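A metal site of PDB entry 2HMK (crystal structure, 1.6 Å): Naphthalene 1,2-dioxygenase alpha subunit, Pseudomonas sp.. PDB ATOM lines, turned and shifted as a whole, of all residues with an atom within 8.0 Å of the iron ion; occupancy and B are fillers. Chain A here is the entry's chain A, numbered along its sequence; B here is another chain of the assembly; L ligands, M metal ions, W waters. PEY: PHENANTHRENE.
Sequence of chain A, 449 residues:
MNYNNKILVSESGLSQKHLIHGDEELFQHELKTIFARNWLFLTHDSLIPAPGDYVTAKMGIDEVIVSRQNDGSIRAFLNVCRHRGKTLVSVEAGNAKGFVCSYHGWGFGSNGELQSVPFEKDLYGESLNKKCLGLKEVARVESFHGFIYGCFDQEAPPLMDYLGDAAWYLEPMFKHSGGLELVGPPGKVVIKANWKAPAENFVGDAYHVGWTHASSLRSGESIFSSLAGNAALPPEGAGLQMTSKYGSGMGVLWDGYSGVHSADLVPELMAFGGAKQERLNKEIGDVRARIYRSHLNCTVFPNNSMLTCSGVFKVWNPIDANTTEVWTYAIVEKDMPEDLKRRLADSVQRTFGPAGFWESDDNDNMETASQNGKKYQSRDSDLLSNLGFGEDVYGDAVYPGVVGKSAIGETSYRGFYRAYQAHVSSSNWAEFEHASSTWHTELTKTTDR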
ATOM      1  N   ASN A 201      -4.427  32.638 -30.782  1.00  0.00           N
ATOM      2  CA  ASN A 201      -5.285  31.456 -30.850  1.00  0.00           C
ATOM      3  C   ASN A 201      -6.369  31.623 -31.921  1.00  0.00           C
ATOM      4  O   ASN A 201      -6.551  30.739 -32.778  1.00  0.00           O
ATOM      5  CB  ASN A 201      -5.880  31.169 -29.477  1.00  0.00           C
ATOM      6  CG  ASN A 201      -6.788  29.977 -29.461  1.00  0.00           C
ATOM      7  OD1 ASN A 201      -7.994  30.129 -29.605  1.00  0.00           O
ATOM      8  ND2 ASN A 201      -6.210  28.787 -29.319  1.00  0.00           N
ATOM      9  N   PHE A 202      -7.064  32.763 -31.904  1.00  0.00           N
ATOM     10  CA  PHE A 202      -8.118  33.025 -32.901  1.00  0.00           C
ATOM     11  C   PHE A 202      -7.567  33.279 -34.297  1.00  0.00           C
ATOM     12  O   PHE A 202      -8.236  32.959 -35.274  1.00  0.00           O
ATOM     13  CB  PHE A 202      -9.024  34.187 -32.491  1.00  0.00           C
ATOM     14  CG  PHE A 202     -10.091  33.797 -31.528  1.00  0.00           C
ATOM     15  CD1 PHE A 202      -9.770  33.343 -30.263  1.00  0.00           C
ATOM     16  CD2 PHE A 202     -11.427  33.870 -31.885  1.00  0.00           C
ATOM     17  CE1 PHE A 202     -10.745  32.964 -29.373  1.00  0.00           C
ATOM     18  CE2 PHE A 202     -12.422  33.482 -30.969  1.00  0.00           C
ATOM     19  CZ  PHE A 202     -12.056  33.017 -29.722  1.00  0.00           C
ATOM     20  N   ASP A 205      -5.179  29.208 -34.984  1.00  0.00           N
ATOM     21  CA  ASP A 205      -5.019  27.973 -34.273  1.00  0.00           C
ATOM     22  C   ASP A 205      -6.146  26.988 -34.457  1.00  0.00           C
ATOM     23  O   ASP A 205      -6.989  26.870 -33.615  1.00  0.00           O
ATOM     24  CB  ASP A 205      -4.783  28.230 -32.796  1.00  0.00           C
ATOM     25  CG  ASP A 205      -4.244  27.020 -32.051  1.00  0.00           C
ATOM     26  OD1 ASP A 205      -3.749  27.290 -30.960  1.00  0.00           O
ATOM     27  OD2 ASP A 205      -4.378  25.876 -32.471  1.00  0.00           O
ATOM     28  N   HIS A 208      -5.479  23.252 -32.168  1.00  0.00           N
ATOM     29  CA  HIS A 208      -5.888  22.991 -30.763  1.00  0.00           C
ATOM     30  C   HIS A 208      -7.308  22.442 -30.626  1.00  0.00           C
ATOM     31  O   HIS A 208      -7.650  21.894 -29.589  1.00  0.00           O
ATOM     32  CB  HIS A 208      -5.743  24.276 -29.902  1.00  0.00           C
ATOM     33  CG  HIS A 208      -6.923  25.198 -29.945  1.00  0.00           C
ATOM     34  ND1 HIS A 208      -7.252  25.951 -31.049  1.00  0.00           N
ATOM     35  CD2 HIS A 208      -7.805  25.537 -28.983  1.00  0.00           C
ATOM     36  CE1 HIS A 208      -8.325  26.676 -30.767  1.00  0.00           C
ATOM     37  NE2 HIS A 208      -8.679  26.437 -29.521  1.00  0.00           N
ATOM     38  N   VAL A 209      -8.146  22.630 -31.644  1.00  0.00           N
ATOM     39  CA  VAL A 209      -9.583  22.490 -31.482  1.00  0.00           C
ATOM     40  C   VAL A 209      -9.978  21.086 -31.019  1.00  0.00           C
ATOM     41  O   VAL A 209     -10.683  20.929 -30.014  1.00  0.00           O
ATOM     42  CB  VAL A 209     -10.354  22.925 -32.744  1.00  0.00           C
ATOM     43  CG1 VAL A 209     -11.865  22.616 -32.618  1.00  0.00           C
ATOM     44  CG2 VAL A 209     -10.120  24.411 -32.970  1.00  0.00           C
ATOM     45  N   THR A 212      -8.061  20.556 -27.216  1.00  0.00           N
ATOM     46  CA  THR A 212      -8.539  21.517 -26.208  1.00  0.00           C
ATOM     47  C   THR A 212     -10.041  21.425 -26.010  1.00  0.00           C
ATOM     48  O   THR A 212     -10.514  21.386 -24.866  1.00  0.00           O
ATOM     49  CB  THR A 212      -8.192  22.989 -26.583  1.00  0.00           C
ATOM     50  OG1 THR A 212      -6.787  23.203 -26.453  1.00  0.00           O
ATOM     51  CG2 THR A 212      -8.923  23.966 -25.654  1.00  0.00           C
ATOM     52  N   HIS A 213     -10.802  21.379 -27.112  1.00  0.00           N
ATOM     53  CA  HIS A 213     -12.264  21.441 -27.055  1.00  0.00           C
ATOM     54  C   HIS A 213     -12.919  20.064 -27.160  1.00  0.00           C
ATOM     55  O   HIS A 213     -14.109  19.975 -27.470  1.00  0.00           O
ATOM     56  CB  HIS A 213     -12.810  22.398 -28.117  1.00  0.00           C
ATOM     57  CG  HIS A 213     -12.383  23.820 -27.943  1.00  0.00           C
ATOM     58  ND1 HIS A 213     -12.780  24.598 -26.866  1.00  0.00           N
ATOM     59  CD2 HIS A 213     -11.566  24.602 -28.685  1.00  0.00           C
ATOM     60  CE1 HIS A 213     -12.227  25.792 -26.963  1.00  0.00           C
ATOM     61  NE2 HIS A 213     -11.487  25.830 -28.059  1.00  0.00           N
ATOM     62  N   LEU A 307     -15.230  34.703 -34.930  1.00  0.00           N
ATOM     63  CA  LEU A 307     -15.547  33.451 -35.620  1.00  0.00           C
ATOM     64  C   LEU A 307     -16.768  33.781 -36.454  1.00  0.00           C
ATOM     65  O   LEU A 307     -17.846  33.934 -35.884  1.00  0.00           O
ATOM     66  CB  LEU A 307     -15.881  32.337 -34.628  1.00  0.00           C
ATOM     67  CG  LEU A 307     -14.832  31.971 -33.590  1.00  0.00           C
ATOM     68  CD1 LEU A 307     -15.313  30.798 -32.727  1.00  0.00           C
ATOM     69  CD2 LEU A 307     -13.478  31.693 -34.230  1.00  0.00           C
ATOM     70  N   PHE A 352     -19.220  30.817 -26.059  1.00  0.00           N
ATOM     71  CA  PHE A 352     -18.009  31.650 -25.944  1.00  0.00           C
ATOM     72  C   PHE A 352     -18.118  32.868 -25.025  1.00  0.00           C
ATOM     73  O   PHE A 352     -17.179  33.683 -24.938  1.00  0.00           O
ATOM     74  CB  PHE A 352     -17.529  32.073 -27.350  1.00  0.00           C
ATOM     75  CG  PHE A 352     -16.721  31.026 -28.021  1.00  0.00           C
ATOM     76  CD1 PHE A 352     -15.337  30.990 -27.869  1.00  0.00           C
ATOM     77  CD2 PHE A 352     -17.318  30.025 -28.751  1.00  0.00           C
ATOM     78  CE1 PHE A 352     -14.587  29.991 -28.444  1.00  0.00           C
ATOM     79  CE2 PHE A 352     -16.560  29.029 -29.330  1.00  0.00           C
ATOM     80  CZ  PHE A 352     -15.217  29.006 -29.178  1.00  0.00           C
ATOM     81  N   TRP A 358     -17.264  26.363 -24.340  1.00  0.00           N
ATOM     82  CA  TRP A 358     -16.088  26.234 -25.221  1.00  0.00           C
ATOM     83  C   TRP A 358     -14.961  27.121 -24.719  1.00  0.00           C
ATOM     84  O   TRP A 358     -13.834  26.659 -24.604  1.00  0.00           O
ATOM     85  CB  TRP A 358     -16.393  26.626 -26.655  1.00  0.00           C
ATOM     86  CG  TRP A 358     -17.281  25.676 -27.413  1.00  0.00           C
ATOM     87  CD1 TRP A 358     -18.587  25.396 -27.140  1.00  0.00           C
ATOM     88  CD2 TRP A 358     -16.955  24.982 -28.627  1.00  0.00           C
ATOM     89  NE1 TRP A 358     -19.096  24.535 -28.099  1.00  0.00           N
ATOM     90  CE2 TRP A 358     -18.112  24.262 -29.015  1.00  0.00           C
ATOM     91  CE3 TRP A 358     -15.797  24.879 -29.402  1.00  0.00           C
ATOM     92  CZ2 TRP A 358     -18.143  23.455 -30.151  1.00  0.00           C
ATOM     93  CZ3 TRP A 358     -15.828  24.072 -30.538  1.00  0.00           C
ATOM     94  CH2 TRP A 358     -16.997  23.361 -30.891  1.00  0.00           C
ATOM     95  N   GLU A 359     -15.265  28.383 -24.462  1.00  0.00           N
ATOM     96  CA  GLU A 359     -14.226  29.351 -24.036  1.00  0.00           C
ATOM     97  C   GLU A 359     -13.540  28.870 -22.769  1.00  0.00           C
ATOM     98  O   GLU A 359     -12.332  29.066 -22.591  1.00  0.00           O
ATOM     99  CB  GLU A 359     -14.846  30.739 -23.815  1.00  0.00           C
ATOM    100  CG  GLU A 359     -13.866  31.832 -23.319  1.00  0.00           C
ATOM    101  CD  GLU A 359     -13.495  32.895 -24.359  1.00  0.00           C
ATOM    102  OE1 GLU A 359     -13.431  32.581 -25.578  1.00  0.00           O
ATOM    103  OE2 GLU A 359     -13.232  34.057 -23.928  1.00  0.00           O
ATOM    104  N   SER A 360     -14.309  28.235 -21.892  1.00  0.00           N
ATOM    105  CA  SER A 360     -13.760  27.750 -20.635  1.00  0.00           C
ATOM    106  C   SER A 360     -12.651  26.738 -20.867  1.00  0.00           C
ATOM    107  O   SER A 360     -11.686  26.678 -20.079  1.00  0.00           O
ATOM    108  CB  SER A 360     -14.875  27.157 -19.761  1.00  0.00           C
ATOM    109  OG  SER A 360     -15.218  25.817 -20.101  1.00  0.00           O
ATOM    110  N   ASP A 361     -12.743  25.964 -21.950  1.00  0.00           N
ATOM    111  CA  ASP A 361     -11.724  24.964 -22.300  1.00  0.00           C
ATOM    112  C   ASP A 361     -10.362  25.600 -22.548  1.00  0.00           C
ATOM    113  O   ASP A 361      -9.344  24.934 -22.402  1.00  0.00           O
ATOM    114  CB  ASP A 361     -12.072  24.204 -23.593  1.00  0.00           C
ATOM    115  CG  ASP A 361     -13.377  23.415 -23.517  1.00  0.00           C
ATOM    116  OD1 ASP A 361     -13.950  23.211 -24.608  1.00  0.00           O
ATOM    117  OD2 ASP A 361     -13.827  22.979 -22.426  1.00  0.00           O
ATOM    118  N   ASP A 362     -10.355  26.863 -22.947  1.00  0.00           N
ATOM    119  CA  ASP A 362      -9.130  27.590 -23.312  1.00  0.00           C
ATOM    120  C   ASP A 362      -8.458  28.281 -22.134  1.00  0.00           C
ATOM    121  O   ASP A 362      -7.291  28.640 -22.226  1.00  0.00           O
ATOM    122  CB  ASP A 362      -9.442  28.694 -24.326  1.00  0.00           C
ATOM    123  CG  ASP A 362      -9.864  28.157 -25.659  1.00  0.00           C
ATOM    124  OD1 ASP A 362     -11.013  28.421 -26.047  1.00  0.00           O
ATOM    125  OD2 ASP A 362      -9.021  27.550 -26.340  1.00  0.00           O
ATOM    126  N   ASN A 363      -9.177  28.476 -21.027  1.00  0.00           N
ATOM    127  CA  ASN A 363      -8.675  29.296 -19.903  1.00  0.00           C
ATOM    128  C   ASN A 363      -7.280  28.889 -19.444  1.00  0.00           C
ATOM    129  O   ASN A 363      -6.366  29.712 -19.425  1.00  0.00           O
ATOM    130  CB  ASN A 363      -9.577  29.221 -18.660  1.00  0.00           C
ATOM    131  CG  ASN A 363     -10.799  30.126 -18.730  1.00  0.00           C
ATOM    132  OD1 ASN A 363     -11.597  30.146 -17.772  1.00  0.00           O
ATOM    133  ND2 ASN A 363     -10.964  30.888 -19.812  1.00  0.00           N
ATOM    134  N   ASN A 365      -5.022  26.957 -20.755  1.00  0.00           N
ATOM    135  CA  ASN A 365      -4.025  27.013 -21.825  1.00  0.00           C
ATOM    136  C   ASN A 365      -3.469  28.435 -21.948  1.00  0.00           C
ATOM    137  O   ASN A 365      -2.253  28.634 -21.968  1.00  0.00           O
ATOM    138  CB  ASN A 365      -4.629  26.607 -23.184  1.00  0.00           C
ATOM    139  CG  ASN A 365      -5.036  25.135 -23.242  1.00  0.00           C
ATOM    140  OD1 ASN A 365      -5.887  24.759 -24.054  1.00  0.00           O
ATOM    141  ND2 ASN A 365      -4.424  24.309 -22.414  1.00  0.00           N
ATOM    142  N   MET A 366      -4.356  29.417 -22.026  1.00  0.00           N
ATOM    143  CA  MET A 366      -4.011  30.835 -22.237  1.00  0.00           C
ATOM    144  C   MET A 366      -3.329  31.428 -21.009  1.00  0.00           C
ATOM    145  O   MET A 366      -2.311  32.153 -21.090  1.00  0.00           O
ATOM    146  CB  MET A 366      -5.275  31.676 -22.473  1.00  0.00           C
ATOM    147  CG  MET A 366      -6.182  31.197 -23.588  1.00  0.00           C
ATOM    148  SD  MET A 366      -5.620  31.695 -25.195  1.00  0.00           S
ATOM    149  CE  MET A 366      -6.927  30.960 -26.208  1.00  0.00           C
ATOM    150  N   TYR B 103      -3.192  21.575 -24.647  1.00  0.00           N
ATOM    151  CA  TYR B 103      -3.421  22.622 -25.643  1.00  0.00           C
ATOM    152  C   TYR B 103      -3.498  21.975 -27.015  1.00  0.00           C
ATOM    153  O   TYR B 103      -4.578  21.937 -27.591  1.00  0.00           O
ATOM    154  CB  TYR B 103      -2.336  23.685 -25.546  1.00  0.00           C
ATOM    155  CG  TYR B 103      -2.671  25.039 -26.136  1.00  0.00           C
ATOM    156  CD1 TYR B 103      -1.883  26.150 -25.839  1.00  0.00           C
ATOM    157  CD2 TYR B 103      -3.743  25.234 -27.014  1.00  0.00           C
ATOM    158  CE1 TYR B 103      -2.178  27.418 -26.380  1.00  0.00           C
ATOM    159  CE2 TYR B 103      -4.033  26.474 -27.568  1.00  0.00           C
ATOM    160  CZ  TYR B 103      -3.250  27.567 -27.251  1.00  0.00           C
ATOM    161  OH  TYR B 103      -3.567  28.803 -27.816  1.00  0.00           O
HETATM  162  C1  PEY L   1     -12.239  28.436 -32.245  1.00  0.00           C
HETATM  163  C2  PEY L   1     -11.464  29.355 -31.572  1.00  0.00           C
HETATM  164  C3  PEY L   1     -10.246  29.724 -32.108  1.00  0.00           C
HETATM  165  C4  PEY L   1      -9.802  29.203 -33.289  1.00  0.00           C
HETATM  166  C5  PEY L   1     -10.590  28.294 -33.957  1.00  0.00           C
HETATM  167  C6  PEY L   1     -11.800  27.914 -33.439  1.00  0.00           C
HETATM  168  C7  PEY L   1     -12.575  27.002 -34.105  1.00  0.00           C
HETATM  169  C8  PEY L   1     -12.170  26.489 -35.310  1.00  0.00           C
HETATM  170  C9  PEY L   1     -10.959  26.852 -35.794  1.00  0.00           C
HETATM  171  C10 PEY L   1     -10.177  27.760 -35.139  1.00  0.00           C
HETATM  172  C11 PEY L   1     -13.779  26.624 -33.574  1.00  0.00           C
HETATM  173  C12 PEY L   1     -14.575  25.710 -34.238  1.00  0.00           C
HETATM  174  C13 PEY L   1     -14.154  25.173 -35.430  1.00  0.00           C
HETATM  175  C14 PEY L   1     -12.952  25.558 -35.985  1.00  0.00           C
HETATM  176 FE    FE M   1     -10.099  27.321 -28.195  1.00  0.00          FE
HETATM  177  O   HOH W   1     -10.336  29.236 -28.824  1.00  0.00           O
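The backbone carbonyl oxygen (O) of Trp 358 sits close to a ring nitrogen (ND1) of His 213 (3.2 Å).
The side-chain carboxylate (OD1) of Asp 361 sits at hydrogen-bond distance from a ring nitrogen (ND1) of His 213, at 2.9 Å.
A ring nitrogen (ND1) of His 208 sits close to the side-chain amide nitrogen (ND2) of Asn 201 (3.5 Å).
O of Asp 205 is in hydrogen-bond range of ND1 of His 208.
The side-chain hydroxyl (OH) of Tyr 103 of chain B lies within hydrogen-bond range of the side-chain amide nitrogen (ND2) of Asn 201.
The side-chain amide nitrogen of Asn 201 is in hydrogen-bond range of the side-chain carboxylate of Asp 205, 3.3 Å away.
The iron ion is bound by water W1, 2.0 Å away.
NE2 of His 213 binds the iron ion, 2.0 Å away.
The iron ion is bound by NE2 of His 208 (2.1 Å).
OD2 of Asp 362 is bound to the iron ion, at 2.2 Å.
The side-chain carboxylate (OD1) of Asp 362 is bound to the iron ion (2.6 Å).
Asn 201 touches the iron ion (OD1 to FE, 3.8 Å).
Four residues have an atom within 4 Å of the iron ion: Asn 201, His 208, His 213 and Asp 362.
The nearest printed residue that does not touch the iron ion is Thr 212 (4.4 Å).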
